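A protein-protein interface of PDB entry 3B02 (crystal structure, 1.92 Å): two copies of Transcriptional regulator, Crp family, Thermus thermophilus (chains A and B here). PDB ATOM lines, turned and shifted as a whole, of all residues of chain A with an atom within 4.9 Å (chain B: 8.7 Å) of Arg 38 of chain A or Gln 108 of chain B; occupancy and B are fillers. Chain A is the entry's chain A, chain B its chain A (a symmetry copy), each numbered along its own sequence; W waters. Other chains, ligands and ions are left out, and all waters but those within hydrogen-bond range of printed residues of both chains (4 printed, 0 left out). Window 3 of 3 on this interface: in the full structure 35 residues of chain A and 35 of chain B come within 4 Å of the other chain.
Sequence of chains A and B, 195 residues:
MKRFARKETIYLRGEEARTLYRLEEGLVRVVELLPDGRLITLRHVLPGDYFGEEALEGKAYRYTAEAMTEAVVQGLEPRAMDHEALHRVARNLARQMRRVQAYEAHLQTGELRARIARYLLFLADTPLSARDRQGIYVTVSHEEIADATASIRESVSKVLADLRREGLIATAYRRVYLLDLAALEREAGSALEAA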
ATOM      1  N   GLU A  32     -10.753  27.050 -23.399  1.00  0.00           N
ATOM      2  CA  GLU A  32     -10.975  27.174 -21.965  1.00  0.00           C
ATOM      3  C   GLU A  32     -11.360  28.622 -21.689  1.00  0.00           C
ATOM      4  O   GLU A  32     -10.764  29.537 -22.255  1.00  0.00           O
ATOM      5  CB  GLU A  32      -9.703  26.825 -21.190  1.00  0.00           C
ATOM      6  CG  GLU A  32      -9.734  27.264 -19.726  1.00  0.00           C
ATOM      7  CD  GLU A  32      -9.417  26.151 -18.757  1.00  0.00           C
ATOM      8  OE1 GLU A  32      -9.852  25.011 -18.984  1.00  0.00           O
ATOM      9  OE2 GLU A  32      -8.753  26.423 -17.738  1.00  0.00           O
ATOM     10  N   LEU A  33     -12.380  28.830 -20.859  1.00  0.00           N
ATOM     11  CA  LEU A  33     -12.774  30.187 -20.477  1.00  0.00           C
ATOM     12  C   LEU A  33     -12.008  30.444 -19.186  1.00  0.00           C
ATOM     13  O   LEU A  33     -12.186  29.712 -18.208  1.00  0.00           O
ATOM     14  CB  LEU A  33     -14.280  30.269 -20.217  1.00  0.00           C
ATOM     15  CG  LEU A  33     -14.775  31.599 -19.641  1.00  0.00           C
ATOM     16  CD1 LEU A  33     -14.398  32.751 -20.572  1.00  0.00           C
ATOM     17  CD2 LEU A  33     -16.284  31.533 -19.442  1.00  0.00           C
ATOM     18  N   LEU A  34     -11.141  31.454 -19.188  1.00  0.00           N
ATOM     19  CA  LEU A  34     -10.332  31.772 -18.010  1.00  0.00           C
ATOM     20  C   LEU A  34     -11.074  32.597 -16.957  1.00  0.00           C
ATOM     21  O   LEU A  34     -12.091  33.234 -17.244  1.00  0.00           O
ATOM     22  CB  LEU A  34      -9.046  32.505 -18.426  1.00  0.00           C
ATOM     23  CG  LEU A  34      -8.083  31.741 -19.347  1.00  0.00           C
ATOM     24  CD1 LEU A  34      -6.868  32.611 -19.656  1.00  0.00           C
ATOM     25  CD2 LEU A  34      -7.656  30.433 -18.692  1.00  0.00           C
ATOM     26  N   ASP A  36     -10.638  35.490 -15.627  1.00  0.00           N
ATOM     27  CA  ASP A  36     -10.865  36.887 -15.997  1.00  0.00           C
ATOM     28  C   ASP A  36     -11.748  37.117 -17.222  1.00  0.00           C
ATOM     29  O   ASP A  36     -11.815  38.236 -17.735  1.00  0.00           O
ATOM     30  CB  ASP A  36      -9.523  37.587 -16.214  1.00  0.00           C
ATOM     31  CG  ASP A  36      -8.640  36.855 -17.201  1.00  0.00           C
ATOM     32  OD1 ASP A  36      -9.130  36.517 -18.299  1.00  0.00           O
ATOM     33  OD2 ASP A  36      -7.455  36.621 -16.881  1.00  0.00           O
ATOM     34  N   GLY A  37     -12.419  36.072 -17.698  1.00  0.00           N
ATOM     35  CA  GLY A  37     -13.286  36.226 -18.853  1.00  0.00           C
ATOM     36  C   GLY A  37     -12.657  35.891 -20.199  1.00  0.00           C
ATOM     37  O   GLY A  37     -13.360  35.726 -21.196  1.00  0.00           O
ATOM     38  N   ARG A  38     -11.334  35.787 -20.233  1.00  0.00           N
ATOM     39  CA  ARG A  38     -10.617  35.468 -21.465  1.00  0.00           C
ATOM     40  C   ARG A  38     -10.901  34.059 -21.976  1.00  0.00           C
ATOM     41  O   ARG A  38     -10.946  33.108 -21.199  1.00  0.00           O
ATOM     42  CB  ARG A  38      -9.105  35.563 -21.243  1.00  0.00           C
ATOM     43  CG  ARG A  38      -8.448  36.888 -21.551  1.00  0.00           C
ATOM     44  CD  ARG A  38      -6.940  36.730 -21.371  1.00  0.00           C
ATOM     45  NE  ARG A  38      -6.621  36.296 -20.012  1.00  0.00           N
ATOM     46  CZ  ARG A  38      -5.535  35.608 -19.663  1.00  0.00           C
ATOM     47  NH1 ARG A  38      -4.632  35.252 -20.571  1.00  0.00           N
ATOM     48  NH2 ARG A  38      -5.352  35.271 -18.393  1.00  0.00           N
ATOM     49  N   LEU A  39     -11.082  33.927 -23.286  1.00  0.00           N
ATOM     50  CA  LEU A  39     -11.267  32.613 -23.879  1.00  0.00           C
ATOM     51  C   LEU A  39      -9.869  32.298 -24.432  1.00  0.00           C
ATOM     52  O   LEU A  39      -9.216  33.175 -24.985  1.00  0.00           O
ATOM     53  CB  LEU A  39     -12.284  32.674 -25.017  1.00  0.00           C
ATOM     54  CG  LEU A  39     -12.780  31.322 -25.531  1.00  0.00           C
ATOM     55  CD1 LEU A  39     -13.453  30.558 -24.393  1.00  0.00           C
ATOM     56  CD2 LEU A  39     -13.764  31.533 -26.672  1.00  0.00           C
ATOM     57  N   ILE A  40      -9.397  31.067 -24.266  1.00  0.00           N
ATOM     58  CA  ILE A  40      -8.075  30.699 -24.767  1.00  0.00           C
ATOM     59  C   ILE A  40      -8.191  29.439 -25.628  1.00  0.00           C
ATOM     60  O   ILE A  40      -8.830  28.476 -25.226  1.00  0.00           O
ATOM     61  CB  ILE A  40      -7.122  30.407 -23.588  1.00  0.00           C
ATOM     62  CG1 ILE A  40      -5.747  29.984 -24.093  1.00  0.00           C
ATOM     63  CG2 ILE A  40      -7.700  29.297 -22.718  1.00  0.00           C
ATOM     64  CD1 ILE A  40      -4.844  29.491 -22.978  1.00  0.00           C
ATOM     65  N   LEU A 107       3.142  30.026 -28.682  1.00  0.00           N
ATOM     66  CA  LEU A 107       2.591  31.073 -27.837  1.00  0.00           C
ATOM     67  C   LEU A 107       3.659  31.859 -27.078  1.00  0.00           C
ATOM     68  O   LEU A 107       3.417  32.992 -26.674  1.00  0.00           O
ATOM     69  CB  LEU A 107       1.592  30.488 -26.841  1.00  0.00           C
ATOM     70  CG  LEU A 107       0.337  29.855 -27.444  1.00  0.00           C
ATOM     71  CD1 LEU A 107      -0.460  29.166 -26.343  1.00  0.00           C
ATOM     72  CD2 LEU A 107      -0.500  30.934 -28.144  1.00  0.00           C
ATOM     73  N   ALA A 150      -1.943  34.313 -27.431  1.00  0.00           N
ATOM     74  CA  ALA A 150      -1.701  34.815 -26.079  1.00  0.00           C
ATOM     75  C   ALA A 150      -1.754  36.346 -26.051  1.00  0.00           C
ATOM     76  O   ALA A 150      -0.823  37.003 -25.590  1.00  0.00           O
ATOM     77  CB  ALA A 150      -0.341  34.328 -25.583  1.00  0.00           C
ATOM     78  N   VAL B 100      -1.713  18.392 -20.486  1.00  0.00           N
ATOM     79  CA  VAL B 100      -0.914  19.399 -21.167  1.00  0.00           C
ATOM     80  C   VAL B 100      -1.752  20.613 -21.536  1.00  0.00           C
ATOM     81  O   VAL B 100      -1.246  21.732 -21.578  1.00  0.00           O
ATOM     82  CB  VAL B 100      -0.180  18.821 -22.424  1.00  0.00           C
ATOM     83  CG1 VAL B 100      -1.155  18.551 -23.556  1.00  0.00           C
ATOM     84  CG2 VAL B 100       0.917  19.791 -22.864  1.00  0.00           C
ATOM     85  N   GLN B 101      -3.040  20.411 -21.789  1.00  0.00           N
ATOM     86  CA  GLN B 101      -3.881  21.557 -22.119  1.00  0.00           C
ATOM     87  C   GLN B 101      -4.105  22.393 -20.854  1.00  0.00           C
ATOM     88  O   GLN B 101      -4.160  23.623 -20.903  1.00  0.00           O
ATOM     89  CB  GLN B 101      -5.195  21.079 -22.730  1.00  0.00           C
ATOM     90  CG  GLN B 101      -4.988  20.560 -24.150  1.00  0.00           C
ATOM     91  CD  GLN B 101      -6.238  19.965 -24.753  1.00  0.00           C
ATOM     92  OE1 GLN B 101      -6.727  20.441 -25.776  1.00  0.00           O
ATOM     93  NE2 GLN B 101      -6.764  18.921 -24.119  1.00  0.00           N
ATOM     94  N   ALA B 102      -4.213  21.718 -19.714  1.00  0.00           N
ATOM     95  CA  ALA B 102      -4.382  22.428 -18.448  1.00  0.00           C
ATOM     96  C   ALA B 102      -3.095  23.195 -18.134  1.00  0.00           C
ATOM     97  O   ALA B 102      -3.131  24.293 -17.580  1.00  0.00           O
ATOM     98  CB  ALA B 102      -4.672  21.453 -17.342  1.00  0.00           C
ATOM     99  N   TYR B 103      -1.957  22.600 -18.484  1.00  0.00           N
ATOM    100  CA  TYR B 103      -0.662  23.236 -18.248  1.00  0.00           C
ATOM    101  C   TYR B 103      -0.577  24.505 -19.101  1.00  0.00           C
ATOM    102  O   TYR B 103      -0.141  25.566 -18.644  1.00  0.00           O
ATOM    103  CB  TYR B 103       0.452  22.248 -18.600  1.00  0.00           C
ATOM    104  CG  TYR B 103       1.837  22.843 -18.586  1.00  0.00           C
ATOM    105  CD1 TYR B 103       2.368  23.412 -17.429  1.00  0.00           C
ATOM    106  CD2 TYR B 103       2.619  22.840 -19.742  1.00  0.00           C
ATOM    107  CE1 TYR B 103       3.655  23.969 -17.423  1.00  0.00           C
ATOM    108  CE2 TYR B 103       3.895  23.386 -19.752  1.00  0.00           C
ATOM    109  CZ  TYR B 103       4.407  23.952 -18.588  1.00  0.00           C
ATOM    110  OH  TYR B 103       5.666  24.509 -18.609  1.00  0.00           O
ATOM    111  N   GLU B 104      -1.003  24.378 -20.354  1.00  0.00           N
ATOM    112  CA  GLU B 104      -1.055  25.494 -21.298  1.00  0.00           C
ATOM    113  C   GLU B 104      -1.840  26.661 -20.716  1.00  0.00           C
ATOM    114  O   GLU B 104      -1.437  27.818 -20.808  1.00  0.00           O
ATOM    115  CB  GLU B 104      -1.837  25.094 -22.536  1.00  0.00           C
ATOM    116  CG  GLU B 104      -1.111  24.461 -23.630  1.00  0.00           C
ATOM    117  CD  GLU B 104      -1.945  24.556 -24.882  1.00  0.00           C
ATOM    118  OE1 GLU B 104      -2.934  23.806 -25.005  1.00  0.00           O
ATOM    119  OE2 GLU B 104      -1.626  25.409 -25.724  1.00  0.00           O
ATOM    120  N   ALA B 105      -3.014  26.346 -20.176  1.00  0.00           N
ATOM    121  CA  ALA B 105      -3.871  27.388 -19.615  1.00  0.00           C
ATOM    122  C   ALA B 105      -3.166  28.064 -18.440  1.00  0.00           C
ATOM    123  O   ALA B 105      -3.188  29.290 -18.307  1.00  0.00           O
ATOM    124  CB  ALA B 105      -5.196  26.793 -19.167  1.00  0.00           C
ATOM    125  N   HIS B 106      -2.525  27.251 -17.608  1.00  0.00           N
ATOM    126  CA  HIS B 106      -1.781  27.740 -16.444  1.00  0.00           C
ATOM    127  C   HIS B 106      -0.742  28.788 -16.850  1.00  0.00           C
ATOM    128  O   HIS B 106      -0.601  29.822 -16.195  1.00  0.00           O
ATOM    129  CB  HIS B 106      -1.107  26.548 -15.743  1.00  0.00           C
ATOM    130  CG  HIS B 106       0.268  26.837 -15.222  1.00  0.00           C
ATOM    131  ND1 HIS B 106       0.498  27.472 -14.019  1.00  0.00           N
ATOM    132  CD2 HIS B 106       1.489  26.573 -15.746  1.00  0.00           C
ATOM    133  CE1 HIS B 106       1.801  27.584 -13.823  1.00  0.00           C
ATOM    134  NE2 HIS B 106       2.427  27.046 -14.858  1.00  0.00           N
ATOM    135  N   LEU B 107      -0.019  28.537 -17.936  1.00  0.00           N
ATOM    136  CA  LEU B 107       0.998  29.482 -18.368  1.00  0.00           C
ATOM    137  C   LEU B 107       0.437  30.869 -18.677  1.00  0.00           C
ATOM    138  O   LEU B 107       1.172  31.851 -18.643  1.00  0.00           O
ATOM    139  CB  LEU B 107       1.736  28.952 -19.596  1.00  0.00           C
ATOM    140  CG  LEU B 107       2.545  27.670 -19.389  1.00  0.00           C
ATOM    141  CD1 LEU B 107       3.066  27.179 -20.735  1.00  0.00           C
ATOM    142  CD2 LEU B 107       3.695  27.937 -18.411  1.00  0.00           C
ATOM    143  N   GLN B 108      -0.860  30.941 -18.964  1.00  0.00           N
ATOM    144  CA  GLN B 108      -1.516  32.204 -19.299  1.00  0.00           C
ATOM    145  C   GLN B 108      -2.512  32.673 -18.232  1.00  0.00           C
ATOM    146  O   GLN B 108      -3.285  33.601 -18.468  1.00  0.00           O
ATOM    147  CB  GLN B 108      -2.237  32.054 -20.652  1.00  0.00           C
ATOM    148  CG  GLN B 108      -1.311  31.621 -21.769  1.00  0.00           C
ATOM    149  CD  GLN B 108      -2.045  31.159 -23.021  1.00  0.00           C
ATOM    150  OE1 GLN B 108      -2.638  31.958 -23.740  1.00  0.00           O
ATOM    151  NE2 GLN B 108      -2.008  29.856 -23.280  1.00  0.00           N
ATOM    152  N   THR B 109      -2.497  32.042 -17.061  1.00  0.00           N
ATOM    153  CA  THR B 109      -3.436  32.424 -16.008  1.00  0.00           C
ATOM    154  C   THR B 109      -2.740  33.053 -14.798  1.00  0.00           C
ATOM    155  O   THR B 109      -1.970  32.392 -14.104  1.00  0.00           O
ATOM    156  CB  THR B 109      -4.255  31.201 -15.521  1.00  0.00           C
ATOM    157  OG1 THR B 109      -4.975  30.634 -16.626  1.00  0.00           O
ATOM    158  CG2 THR B 109      -5.250  31.614 -14.435  1.00  0.00           C
ATOM    159  N   GLY B 110      -3.011  34.338 -14.564  1.00  0.00           N
ATOM    160  CA  GLY B 110      -2.432  35.041 -13.429  1.00  0.00           C
ATOM    161  C   GLY B 110      -1.040  35.612 -13.637  1.00  0.00           C
ATOM    162  O   GLY B 110      -0.364  35.298 -14.618  1.00  0.00           O
ATOM    163  N   GLU B 111      -0.611  36.466 -12.712  1.00  0.00           N
ATOM    164  CA  GLU B 111       0.718  37.059 -12.786  1.00  0.00           C
ATOM    165  C   GLU B 111       1.732  35.988 -12.400  1.00  0.00           C
ATOM    166  O   GLU B 111       1.351  34.895 -11.977  1.00  0.00           O
ATOM    167  CB  GLU B 111       0.836  38.248 -11.830  1.00  0.00           C
ATOM    168  CG  GLU B 111      -0.145  39.374 -12.111  1.00  0.00           C
ATOM    169  CD  GLU B 111       0.089  40.042 -13.455  1.00  0.00           C
ATOM    170  OE1 GLU B 111      -0.602  41.039 -13.744  1.00  0.00           O
ATOM    171  OE2 GLU B 111       0.957  39.571 -14.221  1.00  0.00           O
ATOM    172  N   ARG B 115       1.423  32.031 -10.893  1.00  0.00           N
ATOM    173  CA  ARG B 115       1.914  30.907 -11.692  1.00  0.00           C
ATOM    174  C   ARG B 115       2.969  30.081 -10.950  1.00  0.00           C
ATOM    175  O   ARG B 115       2.997  28.849 -11.045  1.00  0.00           O
ATOM    176  CB  ARG B 115       2.476  31.414 -13.024  1.00  0.00           C
ATOM    177  CG  ARG B 115       1.454  32.208 -13.837  1.00  0.00           C
ATOM    178  CD  ARG B 115       1.769  32.194 -15.339  1.00  0.00           C
ATOM    179  NE  ARG B 115       3.057  32.786 -15.696  1.00  0.00           N
ATOM    180  CZ  ARG B 115       3.297  34.089 -15.818  1.00  0.00           C
ATOM    181  NH1 ARG B 115       2.337  34.982 -15.599  1.00  0.00           N
ATOM    182  NH2 ARG B 115       4.500  34.501 -16.195  1.00  0.00           N
ATOM    183  N   ARG B 118       1.277  28.107  -8.183  1.00  0.00           N
ATOM    184  CA  ARG B 118       0.541  27.006  -8.783  1.00  0.00           C
ATOM    185  C   ARG B 118       1.468  25.875  -9.207  1.00  0.00           C
ATOM    186  O   ARG B 118       1.154  24.697  -9.016  1.00  0.00           O
ATOM    187  CB  ARG B 118      -0.263  27.514  -9.993  1.00  0.00           C
ATOM    188  CG  ARG B 118      -1.351  26.553 -10.489  1.00  0.00           C
ATOM    189  CD  ARG B 118      -2.070  27.128 -11.714  1.00  0.00           C
ATOM    190  NE  ARG B 118      -2.655  28.439 -11.439  1.00  0.00           N
ATOM    191  CZ  ARG B 118      -2.372  29.549 -12.114  1.00  0.00           C
ATOM    192  NH1 ARG B 118      -1.503  29.523 -13.119  1.00  0.00           N
ATOM    193  NH2 ARG B 118      -2.964  30.692 -11.782  1.00  0.00           N
ATOM    194  N   ALA B 148       8.757  26.518 -16.595  1.00  0.00           N
ATOM    195  CA  ALA B 148       7.362  26.082 -16.518  1.00  0.00           C
ATOM    196  C   ALA B 148       6.384  27.162 -16.068  1.00  0.00           C
ATOM    197  O   ALA B 148       5.265  26.854 -15.667  1.00  0.00           O
ATOM    198  CB  ALA B 148       7.241  24.859 -15.595  1.00  0.00           C
ATOM    199  N   THR B 149       6.793  28.423 -16.126  1.00  0.00           N
ATOM    200  CA  THR B 149       5.887  29.497 -15.742  1.00  0.00           C
ATOM    201  C   THR B 149       5.953  30.645 -16.734  1.00  0.00           C
ATOM    202  O   THR B 149       5.509  31.753 -16.437  1.00  0.00           O
ATOM    203  CB  THR B 149       6.208  30.037 -14.337  1.00  0.00           C
ATOM    204  OG1 THR B 149       7.581  30.439 -14.286  1.00  0.00           O
ATOM    205  CG2 THR B 149       5.931  28.965 -13.280  1.00  0.00           C
ATOM    206  N   ALA B 150       6.496  30.371 -17.919  1.00  0.00           N
ATOM    207  CA  ALA B 150       6.610  31.398 -18.953  1.00  0.00           C
ATOM    208  C   ALA B 150       7.312  32.646 -18.407  1.00  0.00           C
ATOM    209  O   ALA B 150       6.794  33.756 -18.501  1.00  0.00           O
ATOM    210  CB  ALA B 150       5.223  31.763 -19.475  1.00  0.00           C
HETATM  211  O   HOH W   1      -6.605  28.581 -16.142  1.00  0.00           O
HETATM  212  O   HOH W   2      -3.645  34.111 -22.869  1.00  0.00           O
HETATM  213  O   HOH W   3      -4.607  36.120 -15.985  1.00  0.00           O
HETATM  214  O   HOH W   4      -3.762  32.403 -26.319  1.00  0.00           O
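The guanidinium group (NH2) of Arg 118 of chain B is in hydrogen-bond range of the backbone carbonyl oxygen (O) of Thr 109 of chain B, 3.0 Å away. The guanidinium group (NH2) of Arg 38 of chain A is in salt-bridge range of the side-chain carboxylate (OD2) of Asp 36 of chain A, 2.9 Å away. The side-chain amide nitrogen of Gln 108 of chain B is in hydrogen-bond range of the backbone carbonyl oxygen of Glu 104 of chain B (3.3 Å). The backbone carbonyl oxygen of Ala 105 of chain B is in hydrogen-bond range of the side-chain hydroxyl of Thr 109 of chain B (2.8 Å). O of Glu 32 of chain A lies within hydrogen-bond range of N of Ile 40 of chain A, at 2.9 Å.
Water W2 lies within hydrogen-bond range of the side-chain amide oxygen of Gln 108 of chain B (2.5 Å) and the guanidinium group of Arg 38 of chain A (2.7 Å). Water W3 lies within hydrogen-bond range of the guanidinium group of Arg 38 of chain A (2.7 Å), the backbone NH of Gly 110 of chain B (2.8 Å) and the side-chain carboxylate of Asp 36 of chain A (3.0 Å). Water W1 bridges the side-chain hydroxyl (OG1) of Thr 109 of chain B (2.7 Å) and the side-chain carboxylate (OE2) of Glu 32 of chain A (3.4 Å). Water W4 bridges the side-chain amide oxygen (OE1) of Gln 108 of chain B (2.8 Å) and the backbone NH (N) of Ala 150 of chain A (2.9 Å).
Glu 32 of chain A touches Ala 105 of chain B. CD1 of Leu 34 of chain A touches O of Gln 108 of chain B (3.9 Å). CD2 of Leu 34 of chain A touches OG1 of Thr 109 of chain B (3.4 Å). Ile 40 of chain A touches Gln 108 of chain B. CD1 of Leu 107 of chain A touches OE2 of Glu 104 of chain B, 3.98 Å away. Gln 108 of chain B touches Leu 107 of chain A. Ala 150 of chain A touches Gln 108 of chain B (CB to OE1, 3.8 Å).
Of chain A, only Leu 34, Arg 38, Ile 40, Leu 107 and Ala 150 come within 4 Å of Gln 108 of chain B. Printed residues of chain B within 4 Å of Glu 32 of chain A: Ala 105. Printed residues of chain B within 4 Å of Leu 34 of chain A: Gln 108 (3.9 Å) and Thr 109 (3.4 Å). Printed residues of chain A within 4 Å of Ala 105 of chain B: Glu 32 (3.9 Å). Glu 111 of chain B touches none of the printed residues of chain A. Val 100 of chain B touches none of the printed residues of chain A. The nearest residue of chain B that does not touch Arg 38 of chain A is Thr 109 of chain B (4.2 Å). The nearest printed residue of chain A that does not touch Gln 108 of chain B is Asp 36 of chain A (5.4 Å). The nearest printed residue of chain B that does not touch Ile 40 of chain A is Ala 105 of chain B (4.1 Å).
The backbone carbonyl oxygen (O) of Gln 108 of chain B sits at hydrogen-bond distance from the guanidinium group (NH2) of Arg 38 of chain A (2.7 Å).
Of the 17 printed residues of chain B, 4 touch a printed residue of chain A. Printed residues of chain A that touch a printed residue of chain B: Glu 32, Leu 34, Arg 38, Ile 40, Leu 107 and Ala 150.
2 positions are printed for both chains. Of the 8 pairs that touch across the chains among the printed residues, none has its exchanged pair printed and touching as well.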
